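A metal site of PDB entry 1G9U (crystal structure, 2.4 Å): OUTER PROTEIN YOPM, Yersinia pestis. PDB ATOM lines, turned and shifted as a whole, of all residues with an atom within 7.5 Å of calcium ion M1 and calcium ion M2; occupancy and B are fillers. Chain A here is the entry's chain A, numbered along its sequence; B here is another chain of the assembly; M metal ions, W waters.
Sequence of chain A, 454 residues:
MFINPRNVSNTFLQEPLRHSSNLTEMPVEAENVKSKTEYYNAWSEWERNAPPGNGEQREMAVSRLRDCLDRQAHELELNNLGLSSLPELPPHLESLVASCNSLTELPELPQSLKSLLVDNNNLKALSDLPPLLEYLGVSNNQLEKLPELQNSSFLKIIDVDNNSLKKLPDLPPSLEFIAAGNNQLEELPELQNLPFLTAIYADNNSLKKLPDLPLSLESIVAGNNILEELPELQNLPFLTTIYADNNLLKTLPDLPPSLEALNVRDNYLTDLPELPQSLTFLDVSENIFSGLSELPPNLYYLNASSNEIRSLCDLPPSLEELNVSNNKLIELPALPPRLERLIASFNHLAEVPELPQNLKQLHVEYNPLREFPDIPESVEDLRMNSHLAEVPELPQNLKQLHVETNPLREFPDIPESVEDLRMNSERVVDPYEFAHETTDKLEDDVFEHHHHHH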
ATOM      1  N   ASN A 224     -10.225   1.065 -23.908  1.00  0.00           N
ATOM      2  CA  ASN A 224      -9.695   0.549 -22.648  1.00  0.00           C
ATOM      3  C   ASN A 224      -8.928  -0.757 -22.792  1.00  0.00           C
ATOM      4  O   ASN A 224      -9.214  -1.735 -22.084  1.00  0.00           O
ATOM      5  CB  ASN A 224     -10.901   0.314 -21.721  1.00  0.00           C
ATOM      6  CG  ASN A 224     -10.614   0.787 -20.298  1.00  0.00           C
ATOM      7  OD1 ASN A 224     -11.216   0.291 -19.330  1.00  0.00           O
ATOM      8  ND2 ASN A 224      -9.652   1.696 -20.127  1.00  0.00           N
ATOM      9  N   ASP A 245     -10.883   4.826 -27.361  1.00  0.00           N
ATOM     10  CA  ASP A 245     -10.687   5.638 -26.189  1.00  0.00           C
ATOM     11  C   ASP A 245      -9.894   4.866 -25.120  1.00  0.00           C
ATOM     12  O   ASP A 245      -9.927   3.626 -25.069  1.00  0.00           O
ATOM     13  CB  ASP A 245     -12.059   5.920 -25.545  1.00  0.00           C
ATOM     14  CG  ASP A 245     -12.854   4.646 -25.367  1.00  0.00           C
ATOM     15  OD1 ASP A 245     -13.267   4.076 -26.391  1.00  0.00           O
ATOM     16  OD2 ASP A 245     -13.094   4.215 -24.214  1.00  0.00           O
ATOM     17  N   ASN A 246      -9.204   5.581 -24.235  1.00  0.00           N
ATOM     18  CA  ASN A 246      -8.532   4.942 -23.128  1.00  0.00           C
ATOM     19  C   ASN A 246      -7.542   3.863 -23.536  1.00  0.00           C
ATOM     20  O   ASN A 246      -7.583   2.715 -23.072  1.00  0.00           O
ATOM     21  CB  ASN A 246      -9.558   4.303 -22.158  1.00  0.00           C
ATOM     22  CG  ASN A 246     -10.352   5.359 -21.409  1.00  0.00           C
ATOM     23  OD1 ASN A 246      -9.856   6.200 -20.656  1.00  0.00           O
ATOM     24  ND2 ASN A 246     -11.669   5.399 -21.597  1.00  0.00           N
ATOM     25  N   ASN A 247      -6.575   4.210 -24.370  1.00  0.00           N
ATOM     26  CA  ASN A 247      -5.501   3.294 -24.712  1.00  0.00           C
ATOM     27  C   ASN A 247      -4.172   4.024 -24.616  1.00  0.00           C
ATOM     28  O   ASN A 247      -3.951   4.909 -23.781  1.00  0.00           O
ATOM     29  CB  ASN A 247      -5.714   2.733 -26.111  1.00  0.00           C
ATOM     30  CG  ASN A 247      -6.711   1.592 -26.190  1.00  0.00           C
ATOM     31  OD1 ASN A 247      -6.407   0.467 -25.759  1.00  0.00           O
ATOM     32  ND2 ASN A 247      -7.890   1.903 -26.748  1.00  0.00           N
ATOM     33  N   ARG A 265     -11.077   9.249 -26.995  1.00  0.00           N
ATOM     34  CA  ARG A 265     -10.979   9.970 -25.729  1.00  0.00           C
ATOM     35  C   ARG A 265      -9.934   9.431 -24.768  1.00  0.00           C
ATOM     36  O   ARG A 265      -9.906   8.216 -24.524  1.00  0.00           O
ATOM     37  CB  ARG A 265     -12.354   9.845 -25.086  1.00  0.00           C
ATOM     38  CG  ARG A 265     -12.331   9.921 -23.566  1.00  0.00           C
ATOM     39  CD  ARG A 265     -13.761  10.214 -23.141  1.00  0.00           C
ATOM     40  NE  ARG A 265     -14.023  10.093 -21.726  1.00  0.00           N
ATOM     41  CZ  ARG A 265     -14.401  11.180 -21.030  1.00  0.00           C
ATOM     42  NH1 ARG A 265     -14.542  12.357 -21.644  1.00  0.00           N
ATOM     43  NH2 ARG A 265     -14.640  11.035 -19.732  1.00  0.00           N
ATOM     44  N   ASP A 266      -9.092  10.294 -24.197  1.00  0.00           N
ATOM     45  CA  ASP A 266      -8.148   9.828 -23.193  1.00  0.00           C
ATOM     46  C   ASP A 266      -7.083   9.007 -23.870  1.00  0.00           C
ATOM     47  O   ASP A 266      -6.891   7.839 -23.548  1.00  0.00           O
ATOM     48  CB  ASP A 266      -8.802   9.040 -22.022  1.00  0.00           C
ATOM     49  CG  ASP A 266      -7.788   8.919 -20.887  1.00  0.00           C
ATOM     50  OD1 ASP A 266      -6.595   9.233 -21.131  1.00  0.00           O
ATOM     51  OD2 ASP A 266      -8.070   8.450 -19.750  1.00  0.00           O
ATOM     52  N   ASN A 267      -6.409   9.710 -24.745  1.00  0.00           N
ATOM     53  CA  ASN A 267      -5.170   9.130 -25.274  1.00  0.00           C
ATOM     54  C   ASN A 267      -4.121  10.256 -25.173  1.00  0.00           C
ATOM     55  O   ASN A 267      -4.327  11.167 -24.350  1.00  0.00           O
ATOM     56  CB  ASN A 267      -5.361   8.589 -26.673  1.00  0.00           C
ATOM     57  CG  ASN A 267      -5.911   7.181 -26.713  1.00  0.00           C
ATOM     58  OD1 ASN A 267      -5.239   6.166 -26.472  1.00  0.00           O
ATOM     59  ND2 ASN A 267      -7.187   7.064 -27.013  1.00  0.00           N
ATOM     60  N   TYR A 268      -3.059  10.214 -25.982  1.00  0.00           N
ATOM     61  CA  TYR A 268      -1.941  11.145 -25.900  1.00  0.00           C
ATOM     62  C   TYR A 268      -1.707  11.839 -27.241  1.00  0.00           C
ATOM     63  O   TYR A 268      -0.593  12.002 -27.726  1.00  0.00           O
ATOM     64  CB  TYR A 268      -0.633  10.466 -25.500  1.00  0.00           C
ATOM     65  CG  TYR A 268       0.372  11.283 -24.702  1.00  0.00           C
ATOM     66  CD1 TYR A 268       0.132  11.655 -23.373  1.00  0.00           C
ATOM     67  CD2 TYR A 268       1.586  11.684 -25.252  1.00  0.00           C
ATOM     68  CE1 TYR A 268       1.062  12.391 -22.650  1.00  0.00           C
ATOM     69  CE2 TYR A 268       2.536  12.417 -24.553  1.00  0.00           C
ATOM     70  CZ  TYR A 268       2.251  12.759 -23.244  1.00  0.00           C
ATOM     71  OH  TYR A 268       3.168  13.489 -22.524  1.00  0.00           O
ATOM     72  N   GLU A 286      -9.842  14.553 -23.442  1.00  0.00           N
ATOM     73  CA  GLU A 286      -8.791  13.958 -22.647  1.00  0.00           C
ATOM     74  C   GLU A 286      -7.594  13.434 -23.438  1.00  0.00           C
ATOM     75  O   GLU A 286      -6.992  12.355 -23.316  1.00  0.00           O
ATOM     76  CB  GLU A 286      -9.430  12.851 -21.824  1.00  0.00           C
ATOM     77  CG  GLU A 286     -10.216  13.276 -20.594  1.00  0.00           C
ATOM     78  CD  GLU A 286     -10.461  12.053 -19.716  1.00  0.00           C
ATOM     79  OE1 GLU A 286      -9.525  11.460 -19.157  1.00  0.00           O
ATOM     80  OE2 GLU A 286     -11.608  11.607 -19.537  1.00  0.00           O
ATOM     81  N   ASN A 287      -7.152  14.318 -24.328  1.00  0.00           N
ATOM     82  CA  ASN A 287      -5.950  14.128 -25.147  1.00  0.00           C
ATOM     83  C   ASN A 287      -5.041  15.292 -24.848  1.00  0.00           C
ATOM     84  O   ASN A 287      -5.055  15.919 -23.775  1.00  0.00           O
ATOM     85  CB  ASN A 287      -6.329  14.068 -26.643  1.00  0.00           C
ATOM     86  CG  ASN A 287      -6.649  12.596 -26.914  1.00  0.00           C
ATOM     87  OD1 ASN A 287      -5.699  11.832 -27.107  1.00  0.00           O
ATOM     88  ND2 ASN A 287      -7.921  12.220 -26.824  1.00  0.00           N
ATOM     89  N   ILE A 288      -4.172  15.672 -25.773  1.00  0.00           N
ATOM     90  CA  ILE A 288      -3.362  16.811 -25.317  1.00  0.00           C
ATOM     91  C   ILE A 288      -3.322  17.889 -26.409  1.00  0.00           C
ATOM     92  O   ILE A 288      -2.240  18.426 -26.713  1.00  0.00           O
ATOM     93  CB  ILE A 288      -1.964  16.325 -24.892  1.00  0.00           C
ATOM     94  CG1 ILE A 288      -1.195  15.600 -26.015  1.00  0.00           C
ATOM     95  CG2 ILE A 288      -1.983  15.408 -23.683  1.00  0.00           C
ATOM     96  CD1 ILE A 288       0.190  15.172 -25.583  1.00  0.00           C
ATOM     97  N   ASN B 287      -2.146  17.051 -16.033  1.00  0.00           N
ATOM     98  CA  ASN B 287      -0.949  17.506 -16.749  1.00  0.00           C
ATOM     99  C   ASN B 287      -0.668  16.473 -17.811  1.00  0.00           C
ATOM    100  O   ASN B 287      -1.542  15.748 -18.314  1.00  0.00           O
ATOM    101  CB  ASN B 287       0.235  17.654 -15.768  1.00  0.00           C
ATOM    102  CG  ASN B 287       0.119  19.078 -15.219  1.00  0.00           C
ATOM    103  OD1 ASN B 287       0.564  19.987 -15.912  1.00  0.00           O
ATOM    104  ND2 ASN B 287      -0.538  19.241 -14.074  1.00  0.00           N
ATOM    105  N   ILE B 288       0.577  16.326 -18.238  1.00  0.00           N
ATOM    106  CA  ILE B 288       0.673  15.288 -19.273  1.00  0.00           C
ATOM    107  C   ILE B 288       1.840  14.342 -18.954  1.00  0.00           C
ATOM    108  O   ILE B 288       2.637  14.013 -19.853  1.00  0.00           O
ATOM    109  CB  ILE B 288       0.787  15.931 -20.661  1.00  0.00           C
ATOM    110  CG1 ILE B 288       1.999  16.875 -20.804  1.00  0.00           C
ATOM    111  CG2 ILE B 288      -0.451  16.710 -21.064  1.00  0.00           C
ATOM    112  CD1 ILE B 288       2.103  17.477 -22.195  1.00  0.00           C
ATOM    113  N   PHE B 289       1.989  13.901 -17.698  1.00  0.00           N
ATOM    114  CA  PHE B 289       3.058  13.009 -17.281  1.00  0.00           C
ATOM    115  C   PHE B 289       2.822  11.569 -17.730  1.00  0.00           C
ATOM    116  O   PHE B 289       1.668  11.140 -17.559  1.00  0.00           O
ATOM    117  CB  PHE B 289       3.198  12.894 -15.741  1.00  0.00           C
ATOM    118  CG  PHE B 289       3.685  14.206 -15.163  1.00  0.00           C
ATOM    119  CD1 PHE B 289       2.753  15.181 -14.849  1.00  0.00           C
ATOM    120  CD2 PHE B 289       5.039  14.424 -14.966  1.00  0.00           C
ATOM    121  CE1 PHE B 289       3.136  16.404 -14.338  1.00  0.00           C
ATOM    122  CE2 PHE B 289       5.420  15.663 -14.493  1.00  0.00           C
ATOM    123  CZ  PHE B 289       4.497  16.643 -14.201  1.00  0.00           C
ATOM    124  N   SER B 306      -5.589  11.783 -13.491  1.00  0.00           N
ATOM    125  CA  SER B 306      -5.795  12.268 -14.828  1.00  0.00           C
ATOM    126  C   SER B 306      -4.554  12.793 -15.538  1.00  0.00           C
ATOM    127  O   SER B 306      -4.656  13.887 -16.086  1.00  0.00           O
ATOM    128  CB  SER B 306      -6.844  13.418 -14.834  1.00  0.00           C
ATOM    129  OG  SER B 306      -8.000  12.773 -14.274  1.00  0.00           O
ATOM    130  N   ASN B 307      -3.496  12.006 -15.530  1.00  0.00           N
ATOM    131  CA  ASN B 307      -2.298  12.182 -16.329  1.00  0.00           C
ATOM    132  C   ASN B 307      -2.284  11.051 -17.360  1.00  0.00           C
ATOM    133  O   ASN B 307      -3.341  10.523 -17.742  1.00  0.00           O
ATOM    134  CB  ASN B 307      -1.020  12.242 -15.513  1.00  0.00           C
ATOM    135  CG  ASN B 307      -0.837  13.689 -15.053  1.00  0.00           C
ATOM    136  OD1 ASN B 307      -0.380  14.571 -15.788  1.00  0.00           O
ATOM    137  ND2 ASN B 307      -1.200  13.915 -13.792  1.00  0.00           N
ATOM    138  N   GLU B 308      -1.115  10.658 -17.836  1.00  0.00           N
ATOM    139  CA  GLU B 308      -1.104   9.534 -18.776  1.00  0.00           C
ATOM    140  C   GLU B 308      -0.128   8.539 -18.150  1.00  0.00           C
ATOM    141  O   GLU B 308       0.739   8.020 -18.841  1.00  0.00           O
ATOM    142  CB  GLU B 308      -0.587   9.962 -20.150  1.00  0.00           C
ATOM    143  CG  GLU B 308      -0.849   8.997 -21.284  1.00  0.00           C
ATOM    144  CD  GLU B 308      -2.301   8.656 -21.526  1.00  0.00           C
ATOM    145  OE1 GLU B 308      -3.249   9.043 -20.816  1.00  0.00           O
ATOM    146  OE2 GLU B 308      -2.513   7.951 -22.537  1.00  0.00           O
ATOM    147  N   ILE B 309      -0.167   8.390 -16.839  1.00  0.00           N
ATOM    148  CA  ILE B 309       0.892   7.586 -16.236  1.00  0.00           C
ATOM    149  C   ILE B 309       0.741   6.084 -16.471  1.00  0.00           C
ATOM    150  O   ILE B 309      -0.353   5.520 -16.358  1.00  0.00           O
ATOM    151  CB  ILE B 309       0.916   7.936 -14.740  1.00  0.00           C
ATOM    152  CG1 ILE B 309       1.269   9.426 -14.583  1.00  0.00           C
ATOM    153  CG2 ILE B 309       1.783   7.005 -13.937  1.00  0.00           C
ATOM    154  CD1 ILE B 309       1.287   9.807 -13.092  1.00  0.00           C
ATOM    155  N   SER B 325      -5.889   8.323  -9.693  1.00  0.00           N
ATOM    156  CA  SER B 325      -7.091   7.918 -10.450  1.00  0.00           C
ATOM    157  C   SER B 325      -6.993   8.258 -11.933  1.00  0.00           C
ATOM    158  O   SER B 325      -6.389   9.260 -12.307  1.00  0.00           O
ATOM    159  CB  SER B 325      -8.290   8.700  -9.859  1.00  0.00           C
ATOM    160  OG  SER B 325      -9.544   8.160 -10.217  1.00  0.00           O
ATOM    161  N   ASN B 326      -7.606   7.460 -12.787  1.00  0.00           N
ATOM    162  CA  ASN B 326      -7.704   7.872 -14.173  1.00  0.00           C
ATOM    163  C   ASN B 326      -6.345   8.080 -14.826  1.00  0.00           C
ATOM    164  O   ASN B 326      -6.128   9.162 -15.382  1.00  0.00           O
ATOM    165  CB  ASN B 326      -8.560   9.143 -14.266  1.00  0.00           C
ATOM    166  CG  ASN B 326      -8.883   9.385 -15.754  1.00  0.00           C
ATOM    167  OD1 ASN B 326      -8.922   8.471 -16.587  1.00  0.00           O
ATOM    168  ND2 ASN B 326      -9.096  10.617 -16.191  1.00  0.00           N
ATOM    169  N   ASN B 327      -5.493   7.046 -14.755  1.00  0.00           N
ATOM    170  CA  ASN B 327      -4.194   7.039 -15.408  1.00  0.00           C
ATOM    171  C   ASN B 327      -4.111   5.809 -16.311  1.00  0.00           C
ATOM    172  O   ASN B 327      -5.141   5.311 -16.703  1.00  0.00           O
ATOM    173  CB  ASN B 327      -2.994   7.080 -14.440  1.00  0.00           C
ATOM    174  CG  ASN B 327      -2.703   8.516 -14.073  1.00  0.00           C
ATOM    175  OD1 ASN B 327      -2.084   9.204 -14.906  1.00  0.00           O
ATOM    176  ND2 ASN B 327      -3.182   8.931 -12.886  1.00  0.00           N
ATOM    177  N   LYS B 328      -2.918   5.321 -16.637  1.00  0.00           N
ATOM    178  CA  LYS B 328      -2.885   4.171 -17.529  1.00  0.00           C
ATOM    179  C   LYS B 328      -2.134   3.057 -16.827  1.00  0.00           C
ATOM    180  O   LYS B 328      -1.325   2.383 -17.468  1.00  0.00           O
ATOM    181  CB  LYS B 328      -2.169   4.542 -18.825  1.00  0.00           C
ATOM    182  CG  LYS B 328      -2.948   5.632 -19.575  1.00  0.00           C
ATOM    183  CD  LYS B 328      -4.246   5.092 -20.112  1.00  0.00           C
ATOM    184  CE  LYS B 328      -5.275   6.043 -20.662  1.00  0.00           C
ATOM    185  NZ  LYS B 328      -4.965   6.887 -21.857  1.00  0.00           N
ATOM    186  N   SER B 345      -8.888   4.391  -8.724  1.00  0.00           N
ATOM    187  CA  SER B 345     -10.020   4.271  -9.619  1.00  0.00           C
ATOM    188  C   SER B 345      -9.634   4.570 -11.070  1.00  0.00           C
ATOM    189  O   SER B 345      -8.764   5.384 -11.376  1.00  0.00           O
ATOM    190  CB  SER B 345     -11.095   5.269  -9.133  1.00  0.00           C
ATOM    191  OG  SER B 345     -11.953   4.578  -8.245  1.00  0.00           O
ATOM    192  N   PHE B 346     -10.335   3.941 -12.013  1.00  0.00           N
ATOM    193  CA  PHE B 346     -10.125   4.090 -13.447  1.00  0.00           C
ATOM    194  C   PHE B 346      -8.698   3.868 -13.920  1.00  0.00           C
ATOM    195  O   PHE B 346      -8.057   4.720 -14.560  1.00  0.00           O
ATOM    196  CB  PHE B 346     -10.569   5.468 -13.997  1.00  0.00           C
ATOM    197  CG  PHE B 346     -12.031   5.735 -13.645  1.00  0.00           C
ATOM    198  CD1 PHE B 346     -13.041   5.287 -14.463  1.00  0.00           C
ATOM    199  CD2 PHE B 346     -12.325   6.392 -12.464  1.00  0.00           C
ATOM    200  CE1 PHE B 346     -14.381   5.535 -14.111  1.00  0.00           C
ATOM    201  CE2 PHE B 346     -13.630   6.617 -12.116  1.00  0.00           C
ATOM    202  CZ  PHE B 346     -14.657   6.167 -12.923  1.00  0.00           C
ATOM    203  N   ASN B 347      -8.216   2.665 -13.654  1.00  0.00           N
ATOM    204  CA  ASN B 347      -6.909   2.340 -14.258  1.00  0.00           C
ATOM    205  C   ASN B 347      -7.067   0.948 -14.894  1.00  0.00           C
ATOM    206  O   ASN B 347      -8.191   0.447 -15.041  1.00  0.00           O
ATOM    207  CB  ASN B 347      -5.790   2.364 -13.232  1.00  0.00           C
ATOM    208  CG  ASN B 347      -5.196   3.755 -13.070  1.00  0.00           C
ATOM    209  OD1 ASN B 347      -4.484   4.224 -13.945  1.00  0.00           O
ATOM    210  ND2 ASN B 347      -5.571   4.345 -11.932  1.00  0.00           N
HETATM  211 CA    CA M   1      -9.533   7.193 -18.546  1.00  0.00          CA
HETATM  212 CA    CA M   2      -4.813  10.483 -19.807  1.00  0.00          CA
HETATM  213  O   HOH W   1      -3.363  12.899 -20.217  1.00  0.00           O
HETATM  214  O   HOH W   2      -6.579  11.909 -19.041  1.00  0.00           O
HETATM  215  O   HOH W   3     -11.196   8.935 -19.168  1.00  0.00           O
HETATM  216  O   HOH W   4      -7.753   5.628 -17.711  1.00  0.00           O
HETATM  217  O   HOH W   5      -4.565  12.039 -22.001  1.00  0.00           O
HETATM  218  O   HOH W   6      -5.581   8.974 -18.063  1.00  0.00           O
HETATM  219  O   HOH W   7     -11.009   5.975 -17.540  1.00  0.00           O
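Water W4 bridges O of Asn 327 of chain B (2.8 Å) and O of Phe 346 of chain B (3.3 Å). Water W5 lies within hydrogen-bond range of the backbone carbonyl oxygen (O) of Asn 267 (2.5 Å) and the backbone carbonyl oxygen (O) of Glu 286 (2.8 Å).
Calcium ion M2 is bound by the side-chain carboxylate of Glu 308 of chain B, water W2, water W6, the backbone carbonyl oxygen of Asn 307 of chain B, the side-chain carboxylate of Asp 266, water W5 and water W1.
Calcium ion M1 is bound by water W7 (2.2 Å), the side-chain carboxylate (OD2) of Asp 266 (2.3 Å), the side-chain amide oxygen (OD1) of Asn 246 (2.4 Å), the side-chain amide oxygen (OD1) of Asn 326 of chain B (2.4 Å), water W3 (2.5 Å) and water W4 (2.5 Å). Calcium ion M1 has six donor atoms within binding distance.
The side-chain carboxylate (OE2) of Glu 308 of chain B lies within salt-bridge range of the side-chain amino group (NZ) of Lys 328 of chain B (2.8 Å). The side-chain amide nitrogen (ND2) of Asn 246 is in hydrogen-bond range of the side-chain carboxylate (OD2) of Asp 245, 3.2 Å away. The backbone NH (N) of Asn 224 lies close to the backbone carbonyl oxygen (O) of Asn 246. OG of Ser 306 of chain B lies within hydrogen-bond range of ND2 of Asn 326 of chain B (3.1 Å). The side-chain carboxylate (OE1) of Glu 286 sits at hydrogen-bond distance from the side-chain amide nitrogen (ND2) of Asn 326 of chain B, 3.1 Å away. OD1 of Asn 307 of chain B is in hydrogen-bond range of N of Phe 289 of chain B (3.1 Å). The backbone NH (N) of Glu 308 of chain B lies within hydrogen-bond range of the side-chain amide oxygen (OD1) of Asn 327 of chain B, at 3.4 Å. O of Asp 266 lies within hydrogen-bond range of NZ of Lys 328 of chain B (2.7 Å).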
